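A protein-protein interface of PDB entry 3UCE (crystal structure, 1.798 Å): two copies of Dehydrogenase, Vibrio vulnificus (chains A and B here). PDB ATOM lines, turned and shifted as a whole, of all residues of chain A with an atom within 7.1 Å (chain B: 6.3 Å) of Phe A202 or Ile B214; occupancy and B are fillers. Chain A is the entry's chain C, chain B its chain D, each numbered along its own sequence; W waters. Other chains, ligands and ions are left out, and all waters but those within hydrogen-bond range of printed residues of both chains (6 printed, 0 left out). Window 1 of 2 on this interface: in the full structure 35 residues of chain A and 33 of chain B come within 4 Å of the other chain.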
ATOM      1  N   ARG A 152     -30.661 -34.113  -1.478  1.00  0.00           N
ATOM      2  CA  ARG A 152     -30.183 -33.375  -0.314  1.00  0.00           C
ATOM      3  C   ARG A 152     -31.021 -32.117  -0.065  1.00  0.00           C
ATOM      4  O   ARG A 152     -31.413 -31.420  -1.007  1.00  0.00           O
ATOM      5  CB  ARG A 152     -28.710 -33.006  -0.506  1.00  0.00           C
ATOM      6  CG  ARG A 152     -27.791 -34.237  -0.592  1.00  0.00           C
ATOM      7  CD  ARG A 152     -26.324 -33.855  -0.767  1.00  0.00           C
ATOM      8  NE  ARG A 152     -26.096 -33.086  -1.986  1.00  0.00           N
ATOM      9  CZ  ARG A 152     -25.935 -31.766  -2.027  1.00  0.00           C
ATOM     10  NH1 ARG A 152     -25.957 -31.039  -0.913  1.00  0.00           N
ATOM     11  NH2 ARG A 152     -25.740 -31.166  -3.189  1.00  0.00           N
ATOM     12  N   ASN A 154     -31.079 -28.620   2.495  1.00  0.00           N
ATOM     13  CA  ASN A 154     -30.439 -27.786   3.516  1.00  0.00           C
ATOM     14  C   ASN A 154     -31.031 -26.397   3.490  1.00  0.00           C
ATOM     15  O   ASN A 154     -31.815 -26.071   2.598  1.00  0.00           O
ATOM     16  CB  ASN A 154     -28.931 -27.650   3.276  1.00  0.00           C
ATOM     17  CG  ASN A 154     -28.219 -28.975   3.254  1.00  0.00           C
ATOM     18  OD1 ASN A 154     -27.996 -29.587   4.299  1.00  0.00           O
ATOM     19  ND2 ASN A 154     -27.847 -29.428   2.056  1.00  0.00           N
ATOM     20  N   ILE A 156     -30.009 -22.055   4.221  1.00  0.00           N
ATOM     21  CA  ILE A 156     -29.073 -20.986   4.528  1.00  0.00           C
ATOM     22  C   ILE A 156     -29.790 -20.015   5.459  1.00  0.00           C
ATOM     23  O   ILE A 156     -30.961 -19.686   5.239  1.00  0.00           O
ATOM     24  CB  ILE A 156     -28.621 -20.237   3.245  1.00  0.00           C
ATOM     25  CG1 ILE A 156     -27.967 -21.207   2.270  1.00  0.00           C
ATOM     26  CG2 ILE A 156     -27.663 -19.083   3.580  1.00  0.00           C
ATOM     27  CD1 ILE A 156     -26.870 -22.072   2.885  1.00  0.00           C
ATOM     28  N   ALA A 197     -24.822 -15.656  -1.154  1.00  0.00           N
ATOM     29  CA  ALA A 197     -24.841 -16.504  -2.339  1.00  0.00           C
ATOM     30  C   ALA A 197     -23.830 -17.645  -2.235  1.00  0.00           C
ATOM     31  O   ALA A 197     -24.118 -18.786  -2.637  1.00  0.00           O
ATOM     32  CB  ALA A 197     -24.551 -15.666  -3.583  1.00  0.00           C
ATOM     33  N   MET A 198     -22.650 -17.320  -1.698  1.00  0.00           N
ATOM     34  CA  MET A 198     -21.547 -18.271  -1.553  1.00  0.00           C
ATOM     35  C   MET A 198     -21.993 -19.490  -0.761  1.00  0.00           C
ATOM     36  O   MET A 198     -21.600 -20.614  -1.060  1.00  0.00           O
ATOM     37  CB  MET A 198     -20.372 -17.598  -0.830  1.00  0.00           C
ATOM     38  CG  MET A 198     -19.094 -18.445  -0.731  1.00  0.00           C
ATOM     39  SD  MET A 198     -17.835 -17.713   0.348  1.00  0.00           S
ATOM     40  CE  MET A 198     -17.726 -16.056  -0.335  1.00  0.00           C
ATOM     41  N   ALA A 199     -22.817 -19.265   0.257  1.00  0.00           N
ATOM     42  CA  ALA A 199     -23.306 -20.365   1.083  1.00  0.00           C
ATOM     43  C   ALA A 199     -24.275 -21.296   0.331  1.00  0.00           C
ATOM     44  O   ALA A 199     -24.222 -22.513   0.503  1.00  0.00           O
ATOM     45  CB  ALA A 199     -23.955 -19.817   2.361  1.00  0.00           C
ATOM     46  N   TYR A 200     -25.165 -20.748  -0.504  1.00  0.00           N
ATOM     47  CA  TYR A 200     -26.010 -21.616  -1.333  1.00  0.00           C
ATOM     48  C   TYR A 200     -25.151 -22.475  -2.279  1.00  0.00           C
ATOM     49  O   TYR A 200     -25.405 -23.663  -2.456  1.00  0.00           O
ATOM     50  CB  TYR A 200     -27.021 -20.813  -2.154  1.00  0.00           C
ATOM     51  CG  TYR A 200     -28.037 -20.057  -1.321  1.00  0.00           C
ATOM     52  CD1 TYR A 200     -29.293 -20.593  -1.050  1.00  0.00           C
ATOM     53  CD2 TYR A 200     -27.733 -18.811  -0.799  1.00  0.00           C
ATOM     54  CE1 TYR A 200     -30.218 -19.889  -0.290  1.00  0.00           C
ATOM     55  CE2 TYR A 200     -28.655 -18.103  -0.041  1.00  0.00           C
ATOM     56  CZ  TYR A 200     -29.886 -18.643   0.216  1.00  0.00           C
ATOM     57  OH  TYR A 200     -30.792 -17.922   0.973  1.00  0.00           O
ATOM     58  N   LEU A 201     -24.144 -21.867  -2.894  1.00  0.00           N
ATOM     59  CA  LEU A 201     -23.256 -22.602  -3.801  1.00  0.00           C
ATOM     60  C   LEU A 201     -22.582 -23.779  -3.088  1.00  0.00           C
ATOM     61  O   LEU A 201     -22.432 -24.862  -3.653  1.00  0.00           O
ATOM     62  CB  LEU A 201     -22.197 -21.663  -4.386  1.00  0.00           C
ATOM     63  CG  LEU A 201     -22.775 -20.565  -5.284  1.00  0.00           C
ATOM     64  CD1 LEU A 201     -21.747 -19.474  -5.578  1.00  0.00           C
ATOM     65  CD2 LEU A 201     -23.298 -21.180  -6.573  1.00  0.00           C
ATOM     66  N   PHE A 202     -22.175 -23.548  -1.847  1.00  0.00           N
ATOM     67  CA  PHE A 202     -21.542 -24.570  -1.026  1.00  0.00           C
ATOM     68  C   PHE A 202     -22.515 -25.718  -0.764  1.00  0.00           C
ATOM     69  O   PHE A 202     -22.156 -26.880  -0.926  1.00  0.00           O
ATOM     70  CB  PHE A 202     -21.031 -23.930   0.273  1.00  0.00           C
ATOM     71  CG  PHE A 202     -20.529 -24.906   1.294  1.00  0.00           C
ATOM     72  CD1 PHE A 202     -19.515 -25.806   0.985  1.00  0.00           C
ATOM     73  CD2 PHE A 202     -21.049 -24.899   2.577  1.00  0.00           C
ATOM     74  CE1 PHE A 202     -19.048 -26.700   1.934  1.00  0.00           C
ATOM     75  CE2 PHE A 202     -20.586 -25.781   3.533  1.00  0.00           C
ATOM     76  CZ  PHE A 202     -19.584 -26.697   3.204  1.00  0.00           C
ATOM     77  N   ALA A 203     -23.754 -25.401  -0.390  1.00  0.00           N
ATOM     78  CA  ALA A 203     -24.747 -26.443  -0.129  1.00  0.00           C
ATOM     79  C   ALA A 203     -25.013 -27.234  -1.410  1.00  0.00           C
ATOM     80  O   ALA A 203     -25.127 -28.456  -1.392  1.00  0.00           O
ATOM     81  CB  ALA A 203     -26.040 -25.830   0.388  1.00  0.00           C
ATOM     82  N   ILE A 204     -25.114 -26.523  -2.525  1.00  0.00           N
ATOM     83  CA  ILE A 204     -25.365 -27.164  -3.808  1.00  0.00           C
ATOM     84  C   ILE A 204     -24.245 -28.138  -4.178  1.00  0.00           C
ATOM     85  O   ILE A 204     -24.489 -29.198  -4.757  1.00  0.00           O
ATOM     86  CB  ILE A 204     -25.517 -26.111  -4.928  1.00  0.00           C
ATOM     87  CG1 ILE A 204     -26.830 -25.345  -4.747  1.00  0.00           C
ATOM     88  CG2 ILE A 204     -25.494 -26.772  -6.301  1.00  0.00           C
ATOM     89  CD1 ILE A 204     -26.882 -24.036  -5.508  1.00  0.00           C
ATOM     90  N   GLN A 205     -23.017 -27.781  -3.832  1.00  0.00           N
ATOM     91  CA  GLN A 205     -21.859 -28.512  -4.331  1.00  0.00           C
ATOM     92  C   GLN A 205     -21.457 -29.694  -3.448  1.00  0.00           C
ATOM     93  O   GLN A 205     -20.800 -30.623  -3.915  1.00  0.00           O
ATOM     94  CB  GLN A 205     -20.674 -27.558  -4.481  1.00  0.00           C
ATOM     95  N   ASN A 206     -21.846 -29.677  -2.178  1.00  0.00           N
ATOM     96  CA  ASN A 206     -21.290 -30.653  -1.244  1.00  0.00           C
ATOM     97  C   ASN A 206     -22.169 -31.882  -1.094  1.00  0.00           C
ATOM     98  O   ASN A 206     -23.203 -31.849  -0.425  1.00  0.00           O
ATOM     99  CB  ASN A 206     -21.031 -30.011   0.122  1.00  0.00           C
ATOM    100  CG  ASN A 206     -20.142 -30.869   1.002  1.00  0.00           C
ATOM    101  OD1 ASN A 206     -20.433 -32.044   1.217  1.00  0.00           O
ATOM    102  ND2 ASN A 206     -19.026 -30.294   1.487  1.00  0.00           N
ATOM    103  N   SER A 207     -21.738 -32.977  -1.706  1.00  0.00           N
ATOM    104  CA  SER A 207     -22.541 -34.191  -1.765  1.00  0.00           C
ATOM    105  C   SER A 207     -22.613 -34.942  -0.436  1.00  0.00           C
ATOM    106  O   SER A 207     -23.283 -35.968  -0.346  1.00  0.00           O
ATOM    107  CB  SER A 207     -21.974 -35.131  -2.826  1.00  0.00           C
ATOM    108  OG  SER A 207     -20.615 -35.414  -2.561  1.00  0.00           O
ATOM    109  N   MET A 209     -23.476 -33.234   2.462  1.00  0.00           N
ATOM    110  CA  MET A 209     -24.215 -32.333   3.354  1.00  0.00           C
ATOM    111  C   MET A 209     -25.734 -32.354   3.105  1.00  0.00           C
ATOM    112  O   MET A 209     -26.217 -32.037   2.019  1.00  0.00           O
ATOM    113  CB  MET A 209     -23.690 -30.885   3.244  1.00  0.00           C
ATOM    114  CG  MET A 209     -24.551 -29.869   4.005  1.00  0.00           C
ATOM    115  SD  MET A 209     -24.366 -28.154   3.422  1.00  0.00           S
ATOM    116  CE  MET A 209     -22.874 -27.787   4.303  1.00  0.00           C
ATOM    117  N   THR A 212     -28.727 -29.725   6.961  1.00  0.00           N
ATOM    118  CA  THR A 212     -27.901 -28.711   7.622  1.00  0.00           C
ATOM    119  C   THR A 212     -28.435 -27.282   7.431  1.00  0.00           C
ATOM    120  O   THR A 212     -28.955 -26.943   6.370  1.00  0.00           O
ATOM    121  CB  THR A 212     -26.455 -28.748   7.075  1.00  0.00           C
ATOM    122  OG1 THR A 212     -25.824 -29.977   7.455  1.00  0.00           O
ATOM    123  CG2 THR A 212     -25.632 -27.587   7.612  1.00  0.00           C
ATOM    124  N   VAL A 213     -28.281 -26.457   8.467  1.00  0.00           N
ATOM    125  CA  VAL A 213     -28.594 -25.039   8.407  1.00  0.00           C
ATOM    126  C   VAL A 213     -27.279 -24.276   8.552  1.00  0.00           C
ATOM    127  O   VAL A 213     -26.576 -24.417   9.544  1.00  0.00           O
ATOM    128  CB  VAL A 213     -29.565 -24.613   9.530  1.00  0.00           C
ATOM    129  CG1 VAL A 213     -29.849 -23.117   9.442  1.00  0.00           C
ATOM    130  CG2 VAL A 213     -30.869 -25.404   9.442  1.00  0.00           C
ATOM    131  N   ILE A 214     -26.924 -23.515   7.526  1.00  0.00           N
ATOM    132  CA  ILE A 214     -25.657 -22.806   7.501  1.00  0.00           C
ATOM    133  C   ILE A 214     -25.899 -21.344   7.865  1.00  0.00           C
ATOM    134  O   ILE A 214     -26.634 -20.661   7.167  1.00  0.00           O
ATOM    135  CB  ILE A 214     -25.068 -22.824   6.091  1.00  0.00           C
ATOM    136  CG1 ILE A 214     -24.712 -24.255   5.679  1.00  0.00           C
ATOM    137  CG2 ILE A 214     -23.847 -21.928   6.024  1.00  0.00           C
ATOM    138  CD1 ILE A 214     -24.133 -24.346   4.262  1.00  0.00           C
ATOM    139  N   ASP A 215     -25.275 -20.873   8.939  1.00  0.00           N
ATOM    140  CA  ASP A 215     -25.406 -19.482   9.350  1.00  0.00           C
ATOM    141  C   ASP A 215     -24.353 -18.616   8.664  1.00  0.00           C
ATOM    142  O   ASP A 215     -23.165 -18.933   8.696  1.00  0.00           O
ATOM    143  CB  ASP A 215     -25.236 -19.358  10.865  1.00  0.00           C
ATOM    144  CG  ASP A 215     -26.396 -19.946  11.636  1.00  0.00           C
ATOM    145  OD1 ASP A 215     -27.564 -19.679  11.270  1.00  0.00           O
ATOM    146  OD2 ASP A 215     -26.142 -20.677  12.615  1.00  0.00           O
ATOM    147  N   ARG B 121     -23.485 -33.540  19.104  1.00  0.00           N
ATOM    148  CA  ARG B 121     -24.940 -33.394  19.165  1.00  0.00           C
ATOM    149  C   ARG B 121     -25.728 -34.657  18.823  1.00  0.00           C
ATOM    150  O   ARG B 121     -26.907 -34.752  19.145  1.00  0.00           O
ATOM    151  CB  ARG B 121     -25.391 -32.220  18.279  1.00  0.00           C
ATOM    152  CG  ARG B 121     -25.071 -30.861  18.918  1.00  0.00           C
ATOM    153  CD  ARG B 121     -24.983 -29.723  17.915  1.00  0.00           C
ATOM    154  NE  ARG B 121     -23.727 -29.734  17.163  1.00  0.00           N
ATOM    155  CZ  ARG B 121     -23.645 -29.761  15.835  1.00  0.00           C
ATOM    156  NH1 ARG B 121     -24.749 -29.784  15.088  1.00  0.00           N
ATOM    157  NH2 ARG B 121     -22.458 -29.760  15.250  1.00  0.00           N
ATOM    158  N   ASN B 154     -14.517 -20.052  13.315  1.00  0.00           N
ATOM    159  CA  ASN B 154     -15.584 -21.005  13.033  1.00  0.00           C
ATOM    160  C   ASN B 154     -15.077 -22.422  13.281  1.00  0.00           C
ATOM    161  O   ASN B 154     -13.895 -22.617  13.552  1.00  0.00           O
ATOM    162  CB  ASN B 154     -16.022 -20.887  11.580  1.00  0.00           C
ATOM    163  CG  ASN B 154     -16.547 -19.511  11.238  1.00  0.00           C
ATOM    164  OD1 ASN B 154     -17.656 -19.146  11.632  1.00  0.00           O
ATOM    165  ND2 ASN B 154     -15.761 -18.747  10.481  1.00  0.00           N
ATOM    166  N   ALA B 155     -15.978 -23.401  13.173  1.00  0.00           N
ATOM    167  CA  ALA B 155     -15.611 -24.797  13.312  1.00  0.00           C
ATOM    168  C   ALA B 155     -16.334 -25.632  12.268  1.00  0.00           C
ATOM    169  O   ALA B 155     -17.485 -25.353  11.915  1.00  0.00           O
ATOM    170  CB  ALA B 155     -15.953 -25.304  14.715  1.00  0.00           C
ATOM    171  N   ILE B 156     -15.634 -26.636  11.761  1.00  0.00           N
ATOM    172  CA  ILE B 156     -16.223 -27.637  10.884  1.00  0.00           C
ATOM    173  C   ILE B 156     -16.512 -28.886  11.720  1.00  0.00           C
ATOM    174  O   ILE B 156     -15.664 -29.335  12.511  1.00  0.00           O
ATOM    175  CB  ILE B 156     -15.261 -28.031   9.725  1.00  0.00           C
ATOM    176  CG1 ILE B 156     -14.738 -26.780   9.010  1.00  0.00           C
ATOM    177  CG2 ILE B 156     -15.954 -28.975   8.729  1.00  0.00           C
ATOM    178  CD1 ILE B 156     -15.839 -25.804   8.591  1.00  0.00           C
ATOM    179  N   SER B 157     -17.694 -29.456  11.520  1.00  0.00           N
ATOM    180  CA  SER B 157     -18.123 -30.623  12.276  1.00  0.00           C
ATOM    181  C   SER B 157     -18.382 -31.784  11.316  1.00  0.00           C
ATOM    182  O   SER B 157     -19.463 -31.905  10.751  1.00  0.00           O
ATOM    183  CB  SER B 157     -19.386 -30.316  13.057  1.00  0.00           C
ATOM    184  OG  SER B 157     -19.742 -31.416  13.859  1.00  0.00           O
ATOM    185  N   PRO B 158     -17.378 -32.642  11.127  1.00  0.00           N
ATOM    186  CA  PRO B 158     -17.506 -33.734  10.153  1.00  0.00           C
ATOM    187  C   PRO B 158     -18.338 -34.908  10.675  1.00  0.00           C
ATOM    188  O   PRO B 158     -18.421 -35.130  11.889  1.00  0.00           O
ATOM    189  CB  PRO B 158     -16.049 -34.191   9.939  1.00  0.00           C
ATOM    190  CG  PRO B 158     -15.180 -33.145  10.603  1.00  0.00           C
ATOM    191  CD  PRO B 158     -16.028 -32.580  11.705  1.00  0.00           C
ATOM    192  N   ASP B 195     -14.651 -33.781   0.602  1.00  0.00           N
ATOM    193  CA  ASP B 195     -15.961 -33.235   0.972  1.00  0.00           C
ATOM    194  C   ASP B 195     -15.843 -32.361   2.217  1.00  0.00           C
ATOM    195  O   ASP B 195     -16.519 -31.346   2.328  1.00  0.00           O
ATOM    196  CB  ASP B 195     -16.988 -34.334   1.274  1.00  0.00           C
ATOM    197  CG  ASP B 195     -17.211 -35.273   0.111  1.00  0.00           C
ATOM    198  OD1 ASP B 195     -17.177 -34.814  -1.053  1.00  0.00           O
ATOM    199  OD2 ASP B 195     -17.437 -36.474   0.379  1.00  0.00           O
ATOM    200  N   ILE B 196     -15.021 -32.778   3.170  1.00  0.00           N
ATOM    201  CA  ILE B 196     -14.865 -32.015   4.407  1.00  0.00           C
ATOM    202  C   ILE B 196     -13.958 -30.801   4.154  1.00  0.00           C
ATOM    203  O   ILE B 196     -14.284 -29.687   4.563  1.00  0.00           O
ATOM    204  CB  ILE B 196     -14.313 -32.881   5.567  1.00  0.00           C
ATOM    205  CG1 ILE B 196     -14.979 -34.263   5.575  1.00  0.00           C
ATOM    206  CG2 ILE B 196     -14.525 -32.178   6.921  1.00  0.00           C
ATOM    207  CD1 ILE B 196     -16.495 -34.221   5.745  1.00  0.00           C
ATOM    208  N   MET B 198     -13.775 -29.028   1.664  1.00  0.00           N
ATOM    209  CA  MET B 198     -14.587 -28.011   0.994  1.00  0.00           C
ATOM    210  C   MET B 198     -15.158 -27.037   2.023  1.00  0.00           C
ATOM    211  O   MET B 198     -15.236 -25.839   1.776  1.00  0.00           O
ATOM    212  CB  MET B 198     -15.745 -28.663   0.220  1.00  0.00           C
ATOM    213  CG  MET B 198     -16.405 -27.753  -0.808  1.00  0.00           C
ATOM    214  SD  MET B 198     -18.003 -28.359  -1.423  1.00  0.00           S
ATOM    215  CE  MET B 198     -17.507 -29.820  -2.339  1.00  0.00           C
ATOM    216  N   ALA B 199     -15.550 -27.565   3.181  1.00  0.00           N
ATOM    217  CA  ALA B 199     -16.148 -26.739   4.231  1.00  0.00           C
ATOM    218  C   ALA B 199     -15.144 -25.765   4.856  1.00  0.00           C
ATOM    219  O   ALA B 199     -15.505 -24.630   5.182  1.00  0.00           O
ATOM    220  CB  ALA B 199     -16.754 -27.626   5.316  1.00  0.00           C
ATOM    221  N   TYR B 200     -13.897 -26.199   5.049  1.00  0.00           N
ATOM    222  CA  TYR B 200     -12.875 -25.287   5.577  1.00  0.00           C
ATOM    223  C   TYR B 200     -12.614 -24.157   4.567  1.00  0.00           C
ATOM    224  O   TYR B 200     -12.429 -23.004   4.948  1.00  0.00           O
ATOM    225  CB  TYR B 200     -11.551 -26.016   5.908  1.00  0.00           C
ATOM    226  CG  TYR B 200     -11.647 -27.066   7.010  1.00  0.00           C
ATOM    227  CD1 TYR B 200     -11.281 -26.777   8.319  1.00  0.00           C
ATOM    228  CD2 TYR B 200     -12.106 -28.346   6.734  1.00  0.00           C
ATOM    229  CE1 TYR B 200     -11.369 -27.746   9.318  1.00  0.00           C
ATOM    230  CE2 TYR B 200     -12.196 -29.310   7.728  1.00  0.00           C
ATOM    231  CZ  TYR B 200     -11.836 -29.006   9.010  1.00  0.00           C
ATOM    232  OH  TYR B 200     -11.934 -29.987   9.979  1.00  0.00           O
ATOM    233  N   PHE B 202     -14.697 -22.876   2.458  1.00  0.00           N
ATOM    234  CA  PHE B 202     -15.862 -22.009   2.595  1.00  0.00           C
ATOM    235  C   PHE B 202     -15.700 -21.067   3.781  1.00  0.00           C
ATOM    236  O   PHE B 202     -15.900 -19.860   3.641  1.00  0.00           O
ATOM    237  CB  PHE B 202     -17.124 -22.863   2.742  1.00  0.00           C
ATOM    238  CG  PHE B 202     -18.368 -22.077   3.053  1.00  0.00           C
ATOM    239  CD1 PHE B 202     -18.816 -21.098   2.188  1.00  0.00           C
ATOM    240  CD2 PHE B 202     -19.101 -22.347   4.198  1.00  0.00           C
ATOM    241  CE1 PHE B 202     -19.981 -20.376   2.465  1.00  0.00           C
ATOM    242  CE2 PHE B 202     -20.253 -21.632   4.493  1.00  0.00           C
ATOM    243  CZ  PHE B 202     -20.696 -20.643   3.622  1.00  0.00           C
ATOM    244  N   ALA B 203     -15.317 -21.604   4.943  1.00  0.00           N
ATOM    245  CA  ALA B 203     -15.180 -20.777   6.146  1.00  0.00           C
ATOM    246  C   ALA B 203     -14.060 -19.743   5.987  1.00  0.00           C
ATOM    247  O   ALA B 203     -14.207 -18.589   6.378  1.00  0.00           O
ATOM    248  CB  ALA B 203     -14.924 -21.653   7.375  1.00  0.00           C
ATOM    249  N   MET B 209     -18.874 -14.648   7.890  1.00  0.00           N
ATOM    250  CA  MET B 209     -19.187 -15.780   8.753  1.00  0.00           C
ATOM    251  C   MET B 209     -18.219 -15.886   9.916  1.00  0.00           C
ATOM    252  O   MET B 209     -17.017 -16.017   9.721  1.00  0.00           O
ATOM    253  CB  MET B 209     -19.174 -17.089   7.970  1.00  0.00           C
ATOM    254  CG  MET B 209     -19.790 -18.231   8.763  1.00  0.00           C
ATOM    255  SD  MET B 209     -19.877 -19.761   7.823  1.00  0.00           S
ATOM    256  CE  MET B 209     -18.150 -20.131   7.781  1.00  0.00           C
ATOM    257  N   THR B 212     -19.649 -19.703  13.680  1.00  0.00           N
ATOM    258  CA  THR B 212     -20.503 -20.721  13.076  1.00  0.00           C
ATOM    259  C   THR B 212     -19.875 -22.113  13.138  1.00  0.00           C
ATOM    260  O   THR B 212     -18.653 -22.260  13.035  1.00  0.00           O
ATOM    261  CB  THR B 212     -20.813 -20.355  11.608  1.00  0.00           C
ATOM    262  OG1 THR B 212     -21.591 -19.146  11.579  1.00  0.00           O
ATOM    263  CG2 THR B 212     -21.593 -21.457  10.900  1.00  0.00           C
ATOM    264  N   VAL B 213     -20.724 -23.124  13.322  1.00  0.00           N
ATOM    265  CA  VAL B 213     -20.306 -24.521  13.260  1.00  0.00           C
ATOM    266  C   VAL B 213     -20.997 -25.127  12.040  1.00  0.00           C
ATOM    267  O   VAL B 213     -22.225 -25.099  11.937  1.00  0.00           O
ATOM    268  CB  VAL B 213     -20.705 -25.310  14.527  1.00  0.00           C
ATOM    269  CG1 VAL B 213     -20.340 -26.786  14.367  1.00  0.00           C
ATOM    270  CG2 VAL B 213     -20.030 -24.728  15.759  1.00  0.00           C
ATOM    271  N   ILE B 214     -20.201 -25.640  11.108  1.00  0.00           N
ATOM    272  CA  ILE B 214     -20.716 -26.155   9.843  1.00  0.00           C
ATOM    273  C   ILE B 214     -20.724 -27.682   9.838  1.00  0.00           C
ATOM    274  O   ILE B 214     -19.662 -28.310   9.856  1.00  0.00           O
ATOM    275  CB  ILE B 214     -19.833 -25.691   8.669  1.00  0.00           C
ATOM    276  CG1 ILE B 214     -19.816 -24.161   8.592  1.00  0.00           C
ATOM    277  CG2 ILE B 214     -20.323 -26.320   7.362  1.00  0.00           C
ATOM    278  CD1 ILE B 214     -18.943 -23.626   7.488  1.00  0.00           C
ATOM    279  N   ASP B 215     -21.912 -28.276   9.780  1.00  0.00           N
ATOM    280  CA  ASP B 215     -22.041 -29.733   9.736  1.00  0.00           C
ATOM    281  C   ASP B 215     -21.899 -30.270   8.314  1.00  0.00           C
ATOM    282  O   ASP B 215     -22.597 -29.831   7.398  1.00  0.00           O
ATOM    283  CB  ASP B 215     -23.398 -30.171  10.269  1.00  0.00           C
ATOM    284  CG  ASP B 215     -23.555 -29.914  11.755  1.00  0.00           C
ATOM    285  OD1 ASP B 215     -22.679 -30.357  12.532  1.00  0.00           O
ATOM    286  OD2 ASP B 215     -24.562 -29.281  12.142  1.00  0.00           O
ATOM    287  N   VAL B 216     -20.995 -31.228   8.146  1.00  0.00           N
ATOM    288  CA  VAL B 216     -20.868 -31.951   6.893  1.00  0.00           C
ATOM    289  C   VAL B 216     -20.819 -33.434   7.260  1.00  0.00           C
ATOM    290  O   VAL B 216     -19.743 -34.013   7.394  1.00  0.00           O
ATOM    291  CB  VAL B 216     -19.597 -31.534   6.141  1.00  0.00           C
ATOM    292  CG1 VAL B 216     -19.531 -32.217   4.792  1.00  0.00           C
ATOM    293  CG2 VAL B 216     -19.565 -30.024   5.970  1.00  0.00           C
HETATM  294  O   HOH W   1     -23.949 -26.166   9.972  1.00  0.00           O
HETATM  295  O   HOH W   2     -18.982 -33.206  -2.624  1.00  0.00           O
HETATM  296  O   HOH W   3     -27.202 -27.404  11.042  1.00  0.00           O
HETATM  297  O   HOH W   4     -24.041 -23.179  10.330  1.00  0.00           O
HETATM  298  O   HOH W   5     -24.686 -32.538   6.668  1.00  0.00           O
HETATM  299  O   HOH W   6     -17.382 -36.416  -3.162  1.00  0.00           O
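The side-chain amide nitrogen of Asn A206 is in hydrogen-bond range of the backbone carbonyl oxygen of Asp B195 (2.8 Å). The side-chain amide nitrogen of Asn A206 lies within hydrogen-bond range of the side-chain sulfur of Met B198, at 3.6 Å. OG1 of Thr A212 lies within hydrogen-bond range of O of Asp B215, 3.2 Å away. O of Asp A215 sits at hydrogen-bond distance from OG1 of Thr B212 (3.3 Å). O of Asp A215 sits close to SD of Met B209 (3.5 Å).
OD1 of Asn A206 lies within hydrogen-bond range of N of Met A209 (3.5 Å). The side-chain amide nitrogen (ND2) of Asn B154 lies within hydrogen-bond range of the backbone carbonyl oxygen (O) of Met B209, at 3.1 Å. N of Ala B155 lies within hydrogen-bond range of O of Thr B212 (2.9 Å). The backbone NH (N) of Ile B214 lies within hydrogen-bond range of the backbone carbonyl oxygen (O) of Ala B155, at 2.8 Å. O of Ile B214 is in hydrogen-bond range of N of Ser B157, 2.8 Å away. The side-chain carboxylate (OD1) of Asp B215 sits close to the side-chain hydroxyl (OG) of Ser B157, at 3.4 Å.
Among the printed residues, pairs that only touch across the chains: Phe A202 with Ala B199, Ala A199 with Phe B202, Phe A202 with Phe B202, Asn A206 with Val B216, Met A209 with Asp B215, Gln A205 with Met B198, Ser A207 with Asp B195, Phe A202 with Met B198, Met A198 with Phe B202, Phe A202 with Ile B214 and Ile A214 with Phe B202.
Phe A202 touches just these residues of chain B: Met B198, Ala B199, Phe B202 and Ile B214. Printed residues of chain A within 4 Å of Thr B212: Asp A215. Printed residues of chain B within 4 Å of Thr A212: Asp B215 (3.2 Å). Of the printed residues of chain B, Gln A205 touches Met B198 (3.7 Å). Printed residues of chain A within 4 Å of Met B198: Phe A202 (3.8 Å), Gln A205 (3.7 Å) and Asn A206 (3.6 Å). Of the printed residues of chain A, Ala B199 touches Phe A202. Asn B154 touches none of the printed residues of chain A. Leu A201 touches none of the printed residues of chain B.
Printed residues of chain B that touch a printed residue of chain A: Asp B195, Met B198, Ala B199, Phe B202, Met B209, Thr B212, Ile B214, Asp B215 and Val B216. Along chain B the printed residues that touch a printed residue of chain A span positions 195 to 216. Of the 19 printed residues of chain A, 10 touch a printed residue of chain B. Printed residues of chain A that touch a printed residue of chain B: Met A198, Ala A199, Phe A202, Gln A205, Asn A206, Ser A207, Met A209, Thr A212, Ile A214 and Asp A215. Hydrophobic or aromatic side chains of chain A that line the printed part of chain B: Met A198, Ala A199, Phe A202, Met A209 and Ile A214. Among the printed residues, 16 pairs touch across the chains.
Ala A199 touches Phe B202, and with the chains exchanged Phe A202 touches Ala B199. Phe A202 touches its own counterpart, Phe B202. Phe A202 touches Ile B214, and with the chains exchanged Ile A214 touches Phe B202. Met A209 touches Asp B215, and with the chains exchanged Asp A215 touches Met B209.
Water W6 lies within hydrogen-bond range of the side-chain carboxylate of Asp B195 (2.7 Å) and the side-chain hydroxyl of Ser A207 (3.4 Å). Water W2 lies within hydrogen-bond range of OG of Ser A207 (2.7 Å), OD1 of Asp B195 (2.9 Å) and O of Gln A205 (3.4 Å). Water W1 lies within hydrogen-bond range of the backbone carbonyl oxygen (O) of Val B213 (2.8 Å), the backbone NH (N) of Asp B215 (2.9 Å) and the backbone carbonyl oxygen (O) of Val A213 (3.2 Å). Water W5 bridges OG1 of Thr A212 (2.9 Å) and O of Asp B215 (3.5 Å). Water W4 lies within hydrogen-bond range of the backbone carbonyl oxygen of Val A213 (2.9 Å), the backbone NH of Asp A215 (3.0 Å) and the backbone carbonyl oxygen of Val B213 (3.1 Å). Water W3 lies within hydrogen-bond range of the backbone NH of Val A213 and the side-chain carboxylate of Asp B215.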
